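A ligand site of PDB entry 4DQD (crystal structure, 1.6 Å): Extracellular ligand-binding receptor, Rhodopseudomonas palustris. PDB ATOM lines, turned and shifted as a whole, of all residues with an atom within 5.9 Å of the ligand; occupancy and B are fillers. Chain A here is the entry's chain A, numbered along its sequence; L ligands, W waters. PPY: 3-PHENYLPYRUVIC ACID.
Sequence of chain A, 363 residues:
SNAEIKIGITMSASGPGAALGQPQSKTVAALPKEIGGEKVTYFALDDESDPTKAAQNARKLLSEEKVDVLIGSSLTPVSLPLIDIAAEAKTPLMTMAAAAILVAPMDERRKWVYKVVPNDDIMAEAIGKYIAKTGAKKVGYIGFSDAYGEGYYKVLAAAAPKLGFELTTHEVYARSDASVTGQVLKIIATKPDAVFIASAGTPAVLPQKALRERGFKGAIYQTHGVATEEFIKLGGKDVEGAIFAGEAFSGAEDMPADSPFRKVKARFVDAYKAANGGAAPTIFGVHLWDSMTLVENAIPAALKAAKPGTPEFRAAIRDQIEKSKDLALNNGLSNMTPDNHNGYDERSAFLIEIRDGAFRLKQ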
ATOM      1  N   LEU A  20     -12.185  14.064 -15.761  1.00  0.00           N
ATOM      2  CA  LEU A  20     -11.995  14.553 -17.121  1.00  0.00           C
ATOM      3  C   LEU A  20     -10.537  14.884 -17.393  1.00  0.00           C
ATOM      4  O   LEU A  20      -9.979  14.498 -18.422  1.00  0.00           O
ATOM      5  CB  LEU A  20     -12.874  15.785 -17.376  1.00  0.00           C
ATOM      6  CG  LEU A  20     -14.392  15.558 -17.350  1.00  0.00           C
ATOM      7  CD1 LEU A  20     -14.911  15.570 -15.903  1.00  0.00           C
ATOM      8  CD2 LEU A  20     -15.105  16.632 -18.165  1.00  0.00           C
ATOM      9  N   SER A  74     -10.547  21.615 -19.102  1.00  0.00           N
ATOM     10  CA  SER A  74     -11.398  20.416 -19.151  1.00  0.00           C
ATOM     11  C   SER A  74     -12.863  20.754 -18.910  1.00  0.00           C
ATOM     12  O   SER A  74     -13.757  19.999 -19.336  1.00  0.00           O
ATOM     13  CB  SER A  74     -10.979  19.446 -18.051  1.00  0.00           C
ATOM     14  OG  SER A  74      -9.604  19.123 -18.123  1.00  0.00           O
ATOM     15  N   LEU A  75     -13.115  21.873 -18.233  1.00  0.00           N
ATOM     16  CA  LEU A  75     -14.449  22.246 -17.785  1.00  0.00           C
ATOM     17  C   LEU A  75     -14.828  23.601 -18.342  1.00  0.00           C
ATOM     18  O   LEU A  75     -13.953  24.443 -18.606  1.00  0.00           O
ATOM     19  CB  LEU A  75     -14.504  22.318 -16.257  1.00  0.00           C
ATOM     20  CG  LEU A  75     -13.843  21.189 -15.475  1.00  0.00           C
ATOM     21  CD1 LEU A  75     -14.000  21.418 -13.957  1.00  0.00           C
ATOM     22  CD2 LEU A  75     -14.434  19.830 -15.870  1.00  0.00           C
ATOM     23  N   THR A  76     -16.122  23.826 -18.481  1.00  0.00           N
ATOM     24  CA  THR A  76     -16.614  25.090 -19.016  1.00  0.00           C
ATOM     25  C   THR A  76     -16.234  26.347 -18.220  1.00  0.00           C
ATOM     26  O   THR A  76     -15.692  27.304 -18.782  1.00  0.00           O
ATOM     27  CB  THR A  76     -18.125  25.024 -19.272  1.00  0.00           C
ATOM     28  OG1 THR A  76     -18.364  24.072 -20.319  1.00  0.00           O
ATOM     29  CG2 THR A  76     -18.670  26.395 -19.700  1.00  0.00           C
ATOM     30  N   PRO A  77     -16.500  26.365 -16.893  1.00  0.00           N
ATOM     31  CA  PRO A  77     -16.207  27.593 -16.143  1.00  0.00           C
ATOM     32  C   PRO A  77     -14.696  27.877 -16.125  1.00  0.00           C
ATOM     33  O   PRO A  77     -14.296  29.038 -16.054  1.00  0.00           O
ATOM     34  CB  PRO A  77     -16.707  27.294 -14.730  1.00  0.00           C
ATOM     35  CG  PRO A  77     -16.976  25.816 -14.686  1.00  0.00           C
ATOM     36  CD  PRO A  77     -17.260  25.384 -16.098  1.00  0.00           C
ATOM     37  N   MET A  96     -11.225  21.930 -24.381  1.00  0.00           N
ATOM     38  CA  MET A  96     -11.655  20.544 -24.232  1.00  0.00           C
ATOM     39  C   MET A  96     -12.994  20.428 -23.510  1.00  0.00           C
ATOM     40  O   MET A  96     -13.447  19.317 -23.218  1.00  0.00           O
ATOM     41  CB  MET A  96     -10.580  19.688 -23.546  1.00  0.00           C
ATOM     42  CG  MET A  96      -9.299  19.603 -24.361  1.00  0.00           C
ATOM     43  SD  MET A  96      -7.929  18.548 -23.479  1.00  0.00           S
ATOM     44  CE  MET A  96      -7.493  19.727 -21.947  1.00  0.00           C
ATOM     45  N   ALA A  97     -13.624  21.572 -23.247  1.00  0.00           N
ATOM     46  CA  ALA A  97     -14.902  21.601 -22.534  1.00  0.00           C
ATOM     47  C   ALA A  97     -16.111  21.634 -23.487  1.00  0.00           C
ATOM     48  O   ALA A  97     -15.947  21.626 -24.705  1.00  0.00           O
ATOM     49  CB  ALA A  97     -14.934  22.772 -21.556  1.00  0.00           C
ATOM     50  N   ALA A  98     -17.331  21.667 -22.935  1.00  0.00           N
ATOM     51  CA  ALA A  98     -18.496  21.309 -23.753  1.00  0.00           C
ATOM     52  C   ALA A  98     -19.509  22.401 -24.068  1.00  0.00           C
ATOM     53  O   ALA A  98     -20.219  22.307 -25.067  1.00  0.00           O
ATOM     54  CB  ALA A  98     -19.225  20.118 -23.104  1.00  0.00           C
ATOM     55  N   ALA A  99     -19.615  23.428 -23.225  1.00  0.00           N
ATOM     56  CA  ALA A  99     -20.708  24.383 -23.401  1.00  0.00           C
ATOM     57  C   ALA A  99     -20.616  25.172 -24.699  1.00  0.00           C
ATOM     58  O   ALA A  99     -19.532  25.584 -25.118  1.00  0.00           O
ATOM     59  CB  ALA A  99     -20.808  25.322 -22.198  1.00  0.00           C
ATOM     60  N   LEU A 102     -18.686  28.523 -25.355  1.00  0.00           N
ATOM     61  CA  LEU A 102     -17.230  28.577 -25.506  1.00  0.00           C
ATOM     62  C   LEU A 102     -16.814  29.011 -26.917  1.00  0.00           C
ATOM     63  O   LEU A 102     -15.724  29.570 -27.091  1.00  0.00           O
ATOM     64  CB  LEU A 102     -16.606  27.239 -25.146  1.00  0.00           C
ATOM     65  CG  LEU A 102     -16.745  26.847 -23.668  1.00  0.00           C
ATOM     66  CD1 LEU A 102     -16.235  25.417 -23.473  1.00  0.00           C
ATOM     67  CD2 LEU A 102     -16.016  27.813 -22.724  1.00  0.00           C
ATOM     68  N   VAL A 117     -15.386  18.915 -28.653  1.00  0.00           N
ATOM     69  CA  VAL A 117     -16.551  18.288 -28.015  1.00  0.00           C
ATOM     70  C   VAL A 117     -17.811  18.922 -28.618  1.00  0.00           C
ATOM     71  O   VAL A 117     -17.897  20.129 -28.728  1.00  0.00           O
ATOM     72  CB  VAL A 117     -16.569  18.532 -26.500  1.00  0.00           C
ATOM     73  CG1 VAL A 117     -17.890  18.005 -25.892  1.00  0.00           C
ATOM     74  CG2 VAL A 117     -15.362  17.853 -25.843  1.00  0.00           C
ATOM     75  N   ASP A 120     -23.145  21.614 -26.400  1.00  0.00           N
ATOM     76  CA  ASP A 120     -24.194  21.066 -25.549  1.00  0.00           C
ATOM     77  C   ASP A 120     -25.608  21.340 -26.054  1.00  0.00           C
ATOM     78  O   ASP A 120     -26.527  20.577 -25.730  1.00  0.00           O
ATOM     79  CB  ASP A 120     -24.056  21.563 -24.114  1.00  0.00           C
ATOM     80  CG  ASP A 120     -22.922  20.884 -23.374  1.00  0.00           C
ATOM     81  OD1 ASP A 120     -22.735  19.666 -23.562  1.00  0.00           O
ATOM     82  OD2 ASP A 120     -22.224  21.566 -22.606  1.00  0.00           O
ATOM     83  N   PHE A 144     -25.532  21.572 -12.450  1.00  0.00           N
ATOM     84  CA  PHE A 144     -24.522  22.448 -11.861  1.00  0.00           C
ATOM     85  C   PHE A 144     -24.957  23.909 -11.953  1.00  0.00           C
ATOM     86  O   PHE A 144     -25.553  24.331 -12.949  1.00  0.00           O
ATOM     87  CB  PHE A 144     -23.207  22.333 -12.636  1.00  0.00           C
ATOM     88  CG  PHE A 144     -22.411  21.069 -12.369  1.00  0.00           C
ATOM     89  CD1 PHE A 144     -22.549  20.355 -11.184  1.00  0.00           C
ATOM     90  CD2 PHE A 144     -21.497  20.621 -13.314  1.00  0.00           C
ATOM     91  CE1 PHE A 144     -21.774  19.212 -10.957  1.00  0.00           C
ATOM     92  CE2 PHE A 144     -20.726  19.486 -13.107  1.00  0.00           C
ATOM     93  CZ  PHE A 144     -20.858  18.768 -11.930  1.00  0.00           C
ATOM     94  N   ASP A 146     -23.544  26.525 -12.886  1.00  0.00           N
ATOM     95  CA  ASP A 146     -22.540  27.173 -13.704  1.00  0.00           C
ATOM     96  C   ASP A 146     -22.971  27.134 -15.164  1.00  0.00           C
ATOM     97  O   ASP A 146     -24.082  26.681 -15.492  1.00  0.00           O
ATOM     98  CB  ASP A 146     -21.154  26.579 -13.488  1.00  0.00           C
ATOM     99  CG  ASP A 146     -21.038  25.125 -13.946  1.00  0.00           C
ATOM    100  OD1 ASP A 146     -21.772  24.726 -14.865  1.00  0.00           O
ATOM    101  OD2 ASP A 146     -20.210  24.398 -13.370  1.00  0.00           O
ATOM    102  N   TYR A 148     -22.080  25.341 -17.635  1.00  0.00           N
ATOM    103  CA  TYR A 148     -22.322  24.017 -18.203  1.00  0.00           C
ATOM    104  C   TYR A 148     -23.730  23.564 -17.897  1.00  0.00           C
ATOM    105  O   TYR A 148     -24.499  23.227 -18.794  1.00  0.00           O
ATOM    106  CB  TYR A 148     -21.314  22.986 -17.671  1.00  0.00           C
ATOM    107  CG  TYR A 148     -21.597  21.590 -18.188  1.00  0.00           C
ATOM    108  CD1 TYR A 148     -21.265  21.241 -19.492  1.00  0.00           C
ATOM    109  CD2 TYR A 148     -22.166  20.621 -17.372  1.00  0.00           C
ATOM    110  CE1 TYR A 148     -21.504  19.970 -19.979  1.00  0.00           C
ATOM    111  CE2 TYR A 148     -22.428  19.328 -17.851  1.00  0.00           C
ATOM    112  CZ  TYR A 148     -22.070  19.014 -19.168  1.00  0.00           C
ATOM    113  OH  TYR A 148     -22.302  17.753 -19.669  1.00  0.00           O
ATOM    114  N   ARG A 175     -20.267  21.825  -7.768  1.00  0.00           N
ATOM    115  CA  ARG A 175     -19.634  20.545  -8.102  1.00  0.00           C
ATOM    116  C   ARG A 175     -19.144  19.729  -6.902  1.00  0.00           C
ATOM    117  O   ARG A 175     -19.258  18.510  -6.900  1.00  0.00           O
ATOM    118  CB  ARG A 175     -18.510  20.720  -9.115  1.00  0.00           C
ATOM    119  CG  ARG A 175     -18.977  21.381 -10.403  1.00  0.00           C
ATOM    120  CD  ARG A 175     -17.939  21.271 -11.524  1.00  0.00           C
ATOM    121  NE  ARG A 175     -18.403  22.020 -12.684  1.00  0.00           N
ATOM    122  CZ  ARG A 175     -18.271  21.624 -13.943  1.00  0.00           C
ATOM    123  NH1 ARG A 175     -17.658  20.477 -14.242  1.00  0.00           N
ATOM    124  NH2 ARG A 175     -18.756  22.382 -14.908  1.00  0.00           N
ATOM    125  N   SER A 199     -24.692  17.394 -15.264  1.00  0.00           N
ATOM    126  CA  SER A 199     -23.505  17.321 -14.426  1.00  0.00           C
ATOM    127  C   SER A 199     -22.352  16.685 -15.221  1.00  0.00           C
ATOM    128  O   SER A 199     -22.503  16.356 -16.408  1.00  0.00           O
ATOM    129  CB  SER A 199     -23.829  16.492 -13.164  1.00  0.00           C
ATOM    130  OG  SER A 199     -22.712  16.427 -12.286  1.00  0.00           O
ATOM    131  N   ALA A 200     -21.192  16.539 -14.590  1.00  0.00           N
ATOM    132  CA  ALA A 200     -20.034  15.964 -15.282  1.00  0.00           C
ATOM    133  C   ALA A 200     -19.076  15.387 -14.280  1.00  0.00           C
ATOM    134  O   ALA A 200     -18.951  15.892 -13.152  1.00  0.00           O
ATOM    135  CB  ALA A 200     -19.319  17.033 -16.116  1.00  0.00           C
ATOM    136  N   THR A 223     -25.904  13.597 -19.051  1.00  0.00           N
ATOM    137  CA  THR A 223     -25.240  14.237 -20.185  1.00  0.00           C
ATOM    138  C   THR A 223     -23.928  13.528 -20.493  1.00  0.00           C
ATOM    139  O   THR A 223     -23.482  12.664 -19.726  1.00  0.00           O
ATOM    140  CB  THR A 223     -24.862  15.695 -19.874  1.00  0.00           C
ATOM    141  OG1 THR A 223     -23.853  15.728 -18.844  1.00  0.00           O
ATOM    142  CG2 THR A 223     -26.085  16.485 -19.425  1.00  0.00           C
ATOM    143  N   HIS A 224     -23.302  13.906 -21.606  1.00  0.00           N
ATOM    144  CA  HIS A 224     -22.010  13.318 -21.955  1.00  0.00           C
ATOM    145  C   HIS A 224     -20.874  13.642 -20.979  1.00  0.00           C
ATOM    146  O   HIS A 224     -19.780  13.098 -21.103  1.00  0.00           O
ATOM    147  CB  HIS A 224     -21.614  13.649 -23.406  1.00  0.00           C
ATOM    148  CG  HIS A 224     -21.517  15.115 -23.699  1.00  0.00           C
ATOM    149  ND1 HIS A 224     -21.066  15.602 -24.914  1.00  0.00           N
ATOM    150  CD2 HIS A 224     -21.818  16.211 -22.950  1.00  0.00           C
ATOM    151  CE1 HIS A 224     -21.074  16.918 -24.894  1.00  0.00           C
ATOM    152  NE2 HIS A 224     -21.527  17.321 -23.718  1.00  0.00           N
ATOM    153  N   GLY A 225     -21.149  14.474 -19.976  1.00  0.00           N
ATOM    154  CA  GLY A 225     -20.210  14.659 -18.891  1.00  0.00           C
ATOM    155  C   GLY A 225     -20.008  13.403 -18.057  1.00  0.00           C
ATOM    156  O   GLY A 225     -19.061  13.333 -17.270  1.00  0.00           O
ATOM    157  N   GLU A 247     -21.143  11.109 -27.684  1.00  0.00           N
ATOM    158  CA  GLU A 247     -20.245  11.036 -28.830  1.00  0.00           C
ATOM    159  C   GLU A 247     -20.129   9.644 -29.429  1.00  0.00           C
ATOM    160  O   GLU A 247     -20.324   8.634 -28.768  1.00  0.00           O
ATOM    161  CB  GLU A 247     -18.848  11.486 -28.406  1.00  0.00           C
ATOM    162  CG  GLU A 247     -18.740  12.996 -28.154  1.00  0.00           C
ATOM    163  CD  GLU A 247     -19.405  13.442 -26.871  1.00  0.00           C
ATOM    164  OE1 GLU A 247     -19.086  12.896 -25.789  1.00  0.00           O
ATOM    165  OE2 GLU A 247     -20.277  14.341 -26.942  1.00  0.00           O
ATOM    166  N   PHE A 284     -12.498  11.059 -21.948  1.00  0.00           N
ATOM    167  CA  PHE A 284     -12.054  12.441 -21.817  1.00  0.00           C
ATOM    168  C   PHE A 284     -10.666  12.704 -22.370  1.00  0.00           C
ATOM    169  O   PHE A 284     -10.368  13.810 -22.823  1.00  0.00           O
ATOM    170  CB  PHE A 284     -12.269  12.946 -20.382  1.00  0.00           C
ATOM    171  CG  PHE A 284     -13.717  12.986 -20.022  1.00  0.00           C
ATOM    172  CD1 PHE A 284     -14.283  11.996 -19.259  1.00  0.00           C
ATOM    173  CD2 PHE A 284     -14.525  13.981 -20.554  1.00  0.00           C
ATOM    174  CE1 PHE A 284     -15.646  12.008 -18.985  1.00  0.00           C
ATOM    175  CE2 PHE A 284     -15.860  14.011 -20.297  1.00  0.00           C
ATOM    176  CZ  PHE A 284     -16.438  13.027 -19.505  1.00  0.00           C
ATOM    177  N   HIS A 287     -10.565  13.999 -25.954  1.00  0.00           N
ATOM    178  CA  HIS A 287     -10.749  15.415 -26.259  1.00  0.00           C
ATOM    179  C   HIS A 287      -9.424  16.134 -26.485  1.00  0.00           C
ATOM    180  O   HIS A 287      -9.357  17.109 -27.231  1.00  0.00           O
ATOM    181  CB  HIS A 287     -11.580  16.084 -25.173  1.00  0.00           C
ATOM    182  CG  HIS A 287     -12.900  15.421 -24.959  1.00  0.00           C
ATOM    183  ND1 HIS A 287     -13.550  14.708 -25.944  1.00  0.00           N
ATOM    184  CD2 HIS A 287     -13.706  15.362 -23.864  1.00  0.00           C
ATOM    185  CE1 HIS A 287     -14.684  14.234 -25.473  1.00  0.00           C
ATOM    186  NE2 HIS A 287     -14.807  14.619 -24.215  1.00  0.00           N
HETATM  187  C1  PPY L   1     -18.026  21.020 -17.659  1.00  0.00           C
HETATM  188  O1  PPY L   1     -18.163  20.221 -16.696  1.00  0.00           O
HETATM  189  O2  PPY L   1     -17.968  22.243 -17.541  1.00  0.00           O
HETATM  190  C2  PPY L   1     -17.984  20.491 -19.016  1.00  0.00           C
HETATM  191  O3  PPY L   1     -17.747  21.264 -19.948  1.00  0.00           O
HETATM  192  C3  PPY L   1     -18.254  19.028 -19.034  1.00  0.00           C
HETATM  193  C1' PPY L   1     -17.898  18.294 -20.260  1.00  0.00           C
HETATM  194  C2' PPY L   1     -18.768  17.387 -20.787  1.00  0.00           C
HETATM  195  C3' PPY L   1     -18.418  16.630 -22.018  1.00  0.00           C
HETATM  196  C4' PPY L   1     -17.198  16.817 -22.621  1.00  0.00           C
HETATM  197  C5' PPY L   1     -16.254  17.806 -22.019  1.00  0.00           C
HETATM  198  C6' PPY L   1     -16.572  18.508 -20.896  1.00  0.00           C
HETATM  199  O   HOH W   1     -17.505  13.572 -23.417  1.00  0.00           O
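Merely in contact with the ligand: Leu 20, Ser 74, Leu 75, Pro 77, Met 96, Ala 97, Val 117, Tyr 148, Ala 200, His 224, Gly 225, Phe 284 and His 287. 16 residues have an atom within 4 Å of the ligand: Leu 20, Ser 74, Leu 75, Thr 76, Pro 77, Met 96, Ala 97, Ala 98, Val 117, Tyr 148, Arg 175, Ala 200, His 224, Gly 225, Phe 284 and His 287. The nearest printed residue that does not touch the ligand is Ala 99 (4.3 Å).
Water W1 lies within hydrogen-bond range of the side-chain carboxylate of Glu 247 (2.9 Å), a ring nitrogen (NE2) of His 287 (3.0 Å) and the backbone carbonyl oxygen of His 224 (3.3 Å).
N of Asp 120 sits at hydrogen-bond distance from O of Ala 98 (3.3 Å). OH of Tyr 148 lies within hydrogen-bond range of N of Gly 225. ND1 of His 224 sits at hydrogen-bond distance from OE2 of Glu 247, at 2.5 Å. OH of Tyr 148 lies within hydrogen-bond range of OG1 of Thr 223, 2.7 Å away. The side-chain hydroxyl (OG1) of Thr 76 is in hydrogen-bond range of the backbone NH (N) of Ala 99, at 3.2 Å. The guanidinium group (NH2) of Arg 175 lies within salt-bridge range of the side-chain carboxylate (OD2) of Asp 146, at 2.9 Å. N of Gly 225 lies close to OG1 of Thr 223, 3.2 Å away. NE2 of His 224 lies within hydrogen-bond range of OD1 of Asp 120 (2.6 Å).
The backbone NH (N) of Thr 76 sits at hydrogen-bond distance from an oxygen (O2) of the ligand (2.6 Å). OG1 of Thr 76 lies within hydrogen-bond range of O3 of the ligand. The backbone NH (N) of Ala 98 is in hydrogen-bond range of an oxygen (O3) of the ligand. O1 of the ligand is in salt-bridge range of NH1 of Arg 175 (2.5 Å).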
